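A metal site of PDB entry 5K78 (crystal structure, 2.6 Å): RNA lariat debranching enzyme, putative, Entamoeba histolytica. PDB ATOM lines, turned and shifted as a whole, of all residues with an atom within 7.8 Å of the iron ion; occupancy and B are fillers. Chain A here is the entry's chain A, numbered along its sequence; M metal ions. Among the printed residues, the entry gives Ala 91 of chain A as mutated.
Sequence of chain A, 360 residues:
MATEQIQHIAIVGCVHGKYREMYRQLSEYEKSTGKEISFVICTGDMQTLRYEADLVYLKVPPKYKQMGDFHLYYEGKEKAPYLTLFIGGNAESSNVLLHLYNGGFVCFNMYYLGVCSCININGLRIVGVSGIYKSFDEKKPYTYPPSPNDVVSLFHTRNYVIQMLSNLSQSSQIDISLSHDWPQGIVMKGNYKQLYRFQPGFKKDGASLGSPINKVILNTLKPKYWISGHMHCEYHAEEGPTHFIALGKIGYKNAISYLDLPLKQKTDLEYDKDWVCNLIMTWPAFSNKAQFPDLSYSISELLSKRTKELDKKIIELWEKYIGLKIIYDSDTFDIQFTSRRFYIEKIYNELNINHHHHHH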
ATOM      1  N   CYS A  14      -4.184  17.795 -24.615  1.00  0.00           N
ATOM      2  CA  CYS A  14      -3.309  18.529 -25.521  1.00  0.00           C
ATOM      3  C   CYS A  14      -4.099  19.033 -26.711  1.00  0.00           C
ATOM      4  O   CYS A  14      -4.852  18.274 -27.331  1.00  0.00           O
ATOM      5  CB  CYS A  14      -2.153  17.638 -25.992  1.00  0.00           C
ATOM      6  SG  CYS A  14      -1.142  16.927 -24.672  1.00  0.00           S
ATOM      7  N   HIS A  16      -2.405  21.249 -29.269  1.00  0.00           N
ATOM      8  CA  HIS A  16      -1.428  21.220 -30.356  1.00  0.00           C
ATOM      9  C   HIS A  16      -1.903  22.044 -31.556  1.00  0.00           C
ATOM     10  O   HIS A  16      -1.770  21.630 -32.713  1.00  0.00           O
ATOM     11  CB  HIS A  16      -1.103  19.789 -30.777  1.00  0.00           C
ATOM     12  CG  HIS A  16      -0.203  19.065 -29.829  1.00  0.00           C
ATOM     13  ND1 HIS A  16       1.150  19.331 -29.724  1.00  0.00           N
ATOM     14  CD2 HIS A  16      -0.453  18.076 -28.929  1.00  0.00           C
ATOM     15  CE1 HIS A  16       1.683  18.548 -28.815  1.00  0.00           C
ATOM     16  NE2 HIS A  16       0.733  17.778 -28.307  1.00  0.00           N
ATOM     17  N   THR A  43      -4.846  21.538 -20.645  1.00  0.00           N
ATOM     18  CA  THR A  43      -3.700  21.091 -19.864  1.00  0.00           C
ATOM     19  C   THR A  43      -2.357  21.386 -20.535  1.00  0.00           C
ATOM     20  O   THR A  43      -1.341  20.827 -20.113  1.00  0.00           O
ATOM     21  CB  THR A  43      -3.805  19.589 -19.588  1.00  0.00           C
ATOM     22  OG1 THR A  43      -3.781  18.865 -20.825  1.00  0.00           O
ATOM     23  CG2 THR A  43      -5.096  19.283 -18.843  1.00  0.00           C
ATOM     24  N   GLY A  44      -2.328  22.233 -21.554  1.00  0.00           N
ATOM     25  CA  GLY A  44      -1.085  22.686 -22.141  1.00  0.00           C
ATOM     26  C   GLY A  44      -0.937  22.238 -23.578  1.00  0.00           C
ATOM     27  O   GLY A  44      -1.832  21.644 -24.180  1.00  0.00           O
ATOM     28  N   ASP A  45       0.251  22.527 -24.134  1.00  0.00           N
ATOM     29  CA  ASP A  45       0.549  22.312 -25.546  1.00  0.00           C
ATOM     30  C   ASP A  45      -0.450  23.062 -26.429  1.00  0.00           C
ATOM     31  O   ASP A  45      -1.147  22.481 -27.265  1.00  0.00           O
ATOM     32  CB  ASP A  45       0.608  20.826 -25.889  1.00  0.00           C
ATOM     33  CG  ASP A  45       1.903  20.173 -25.463  1.00  0.00           C
ATOM     34  OD1 ASP A  45       2.643  20.798 -24.663  1.00  0.00           O
ATOM     35  OD2 ASP A  45       2.190  19.044 -25.915  1.00  0.00           O
ATOM     36  N   GLY A  88       0.596  26.132 -19.666  1.00  0.00           N
ATOM     37  CA  GLY A  88       1.582  25.883 -20.701  1.00  0.00           C
ATOM     38  C   GLY A  88       2.128  24.473 -20.618  1.00  0.00           C
ATOM     39  O   GLY A  88       2.251  23.892 -19.535  1.00  0.00           O
ATOM     40  N   GLY A  89       2.442  23.904 -21.777  1.00  0.00           N
ATOM     41  CA  GLY A  89       3.061  22.593 -21.848  1.00  0.00           C
ATOM     42  C   GLY A  89       4.503  22.665 -22.314  1.00  0.00           C
ATOM     43  O   GLY A  89       5.272  23.503 -21.841  1.00  0.00           O
ATOM     44  N   ASN A  90       4.877  21.779 -23.249  1.00  0.00           N
ATOM     45  CA  ASN A  90       6.199  21.805 -23.851  1.00  0.00           C
ATOM     46  C   ASN A  90       6.202  22.284 -25.291  1.00  0.00           C
ATOM     47  O   ASN A  90       7.238  22.771 -25.761  1.00  0.00           O
ATOM     48  CB  ASN A  90       6.853  20.419 -23.780  1.00  0.00           C
ATOM     49  CG  ASN A  90       5.999  19.350 -24.430  1.00  0.00           C
ATOM     50  OD1 ASN A  90       5.141  18.744 -23.789  1.00  0.00           O
ATOM     51  ND2 ASN A  90       6.231  19.101 -25.716  1.00  0.00           N
ATOM     52  N   ALA A  91       5.079  22.145 -25.999  1.00  0.00           N
ATOM     53  CA  ALA A  91       4.936  22.663 -27.356  1.00  0.00           C
ATOM     54  C   ALA A  91       4.162  23.977 -27.242  1.00  0.00           C
ATOM     55  O   ALA A  91       2.934  24.010 -27.343  1.00  0.00           O
ATOM     56  CB  ALA A  91       4.227  21.658 -28.254  1.00  0.00           C
ATOM     57  N   GLU A  92       4.888  25.062 -27.016  1.00  0.00           N
ATOM     58  CA  GLU A  92       4.279  26.360 -26.774  1.00  0.00           C
ATOM     59  C   GLU A  92       5.060  27.436 -27.510  1.00  0.00           C
ATOM     60  O   GLU A  92       6.220  27.254 -27.876  1.00  0.00           O
ATOM     61  CB  GLU A  92       4.247  26.702 -25.274  1.00  0.00           C
ATOM     62  CG  GLU A  92       3.472  25.719 -24.410  1.00  0.00           C
ATOM     63  CD  GLU A  92       1.971  25.867 -24.551  1.00  0.00           C
ATOM     64  OE1 GLU A  92       1.526  26.781 -25.275  1.00  0.00           O
ATOM     65  OE2 GLU A  92       1.242  25.063 -23.926  1.00  0.00           O
ATOM     66  N   GLY A 131       4.362  23.788 -17.768  1.00  0.00           N
ATOM     67  CA  GLY A 131       5.630  23.200 -18.150  1.00  0.00           C
ATOM     68  C   GLY A 131       5.756  21.718 -17.845  1.00  0.00           C
ATOM     69  O   GLY A 131       4.857  21.073 -17.294  1.00  0.00           O
ATOM     70  N   ILE A 132       6.908  21.183 -18.228  1.00  0.00           N
ATOM     71  CA  ILE A 132       7.285  19.811 -17.913  1.00  0.00           C
ATOM     72  C   ILE A 132       8.595  19.846 -17.140  1.00  0.00           C
ATOM     73  O   ILE A 132       9.366  20.813 -17.216  1.00  0.00           O
ATOM     74  CB  ILE A 132       7.427  18.938 -19.178  1.00  0.00           C
ATOM     75  CG1 ILE A 132       8.610  19.406 -20.031  1.00  0.00           C
ATOM     76  CG2 ILE A 132       6.134  18.962 -19.997  1.00  0.00           C
ATOM     77  CD1 ILE A 132       8.859  18.554 -21.257  1.00  0.00           C
ATOM     78  N   HIS A 180       0.815  19.809 -16.674  1.00  0.00           N
ATOM     79  CA  HIS A 180       0.930  19.229 -18.017  1.00  0.00           C
ATOM     80  C   HIS A 180       1.372  17.776 -17.900  1.00  0.00           C
ATOM     81  O   HIS A 180       0.588  16.856 -18.176  1.00  0.00           O
ATOM     82  CB  HIS A 180       1.898  20.046 -18.883  1.00  0.00           C
ATOM     83  CG  HIS A 180       1.840  19.687 -20.328  1.00  0.00           C
ATOM     84  ND1 HIS A 180       0.688  19.808 -21.078  1.00  0.00           N
ATOM     85  CD2 HIS A 180       2.785  19.204 -21.170  1.00  0.00           C
ATOM     86  CE1 HIS A 180       0.923  19.411 -22.317  1.00  0.00           C
ATOM     87  NE2 HIS A 180       2.194  19.037 -22.402  1.00  0.00           N
ATOM     88  N   ASP A 181       2.619  17.547 -17.493  1.00  0.00           N
ATOM     89  CA  ASP A 181       3.056  16.187 -17.205  1.00  0.00           C
ATOM     90  C   ASP A 181       2.460  15.712 -15.882  1.00  0.00           C
ATOM     91  O   ASP A 181       2.088  16.513 -15.019  1.00  0.00           O
ATOM     92  CB  ASP A 181       4.587  16.101 -17.188  1.00  0.00           C
ATOM     93  CG  ASP A 181       5.224  17.199 -16.370  1.00  0.00           C
ATOM     94  OD1 ASP A 181       4.525  18.167 -15.994  1.00  0.00           O
ATOM     95  OD2 ASP A 181       6.442  17.106 -16.095  1.00  0.00           O
ATOM     96  N   GLY A 229      -2.128  16.198 -18.896  1.00  0.00           N
ATOM     97  CA  GLY A 229      -2.104  15.699 -20.249  1.00  0.00           C
ATOM     98  C   GLY A 229      -0.757  15.169 -20.674  1.00  0.00           C
ATOM     99  O   GLY A 229      -0.233  14.237 -20.046  1.00  0.00           O
ATOM    100  N   HIS A 230      -0.196  15.729 -21.750  1.00  0.00           N
ATOM    101  CA  HIS A 230       1.170  15.466 -22.180  1.00  0.00           C
ATOM    102  C   HIS A 230       1.361  14.051 -22.736  1.00  0.00           C
ATOM    103  O   HIS A 230       2.084  13.869 -23.723  1.00  0.00           O
ATOM    104  CB  HIS A 230       2.160  15.733 -21.040  1.00  0.00           C
ATOM    105  CG  HIS A 230       3.604  15.572 -21.424  1.00  0.00           C
ATOM    106  ND1 HIS A 230       4.151  16.191 -22.527  1.00  0.00           N
ATOM    107  CD2 HIS A 230       4.606  14.885 -20.844  1.00  0.00           C
ATOM    108  CE1 HIS A 230       5.429  15.878 -22.616  1.00  0.00           C
ATOM    109  NE2 HIS A 230       5.736  15.087 -21.595  1.00  0.00           N
ATOM    110  N   MET A 231       0.717  13.063 -22.121  1.00  0.00           N
ATOM    111  CA  MET A 231       0.961  11.664 -22.463  1.00  0.00           C
ATOM    112  C   MET A 231       0.092  11.147 -23.609  1.00  0.00           C
ATOM    113  O   MET A 231       0.287  10.007 -24.029  1.00  0.00           O
ATOM    114  CB  MET A 231       0.729  10.786 -21.237  1.00  0.00           C
ATOM    115  CG  MET A 231       1.591  11.159 -20.038  1.00  0.00           C
ATOM    116  SD  MET A 231       3.356  11.205 -20.411  1.00  0.00           S
ATOM    117  CE  MET A 231       3.744   9.459 -20.331  1.00  0.00           C
ATOM    118  N   HIS A 232      -0.846  11.950 -24.117  1.00  0.00           N
ATOM    119  CA  HIS A 232      -1.659  11.584 -25.279  1.00  0.00           C
ATOM    120  C   HIS A 232      -2.453  10.305 -25.025  1.00  0.00           C
ATOM    121  O   HIS A 232      -2.628   9.476 -25.922  1.00  0.00           O
ATOM    122  CB  HIS A 232      -0.806  11.445 -26.541  1.00  0.00           C
ATOM    123  CG  HIS A 232      -0.117  12.701 -26.953  1.00  0.00           C
ATOM    124  ND1 HIS A 232       0.959  12.713 -27.826  1.00  0.00           N
ATOM    125  CD2 HIS A 232      -0.338  14.002 -26.632  1.00  0.00           C
ATOM    126  CE1 HIS A 232       1.361  13.949 -28.022  1.00  0.00           C
ATOM    127  NE2 HIS A 232       0.592  14.747 -27.302  1.00  0.00           N
HETATM  128 FE    FE M   1       3.141  17.748 -24.022  1.00  0.00          FE
HETATM  129 ZN    ZN M   2       0.940  16.700 -26.247  1.00  0.00          ZN
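The iron ion is bound by the side-chain amide oxygen (OD1) of Asn 90, at 2.2 Å. The iron ion is bound by NE2 of His 180 (2.3 Å). ND1 of His 230 binds the iron ion (2.4 Å). OD2 of Asp 45 binds the iron ion, at 2.5 Å.
The backbone carbonyl oxygen (O) of His 180 lies within hydrogen-bond range of the backbone NH (N) of Gly 229. A ring nitrogen (ND1) of His 180 is in hydrogen-bond range of the backbone carbonyl oxygen (O) of Thr 43 (2.5 Å). The side-chain sulfur (SG) of Cys 14 sits close to the backbone NH (N) of His 230. O of Asp 45 lies within hydrogen-bond range of N of His 16 (2.7 Å). The side-chain carboxylate (OD1) of Asp 45 sits at hydrogen-bond distance from the backbone NH (N) of Ala 91. The backbone NH (N) of Asp 45 is in hydrogen-bond range of the side-chain carboxylate (OE2) of Glu 92.
Within 4 Å of the iron ion: Asp 45, Asn 90, His 180 and His 230.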
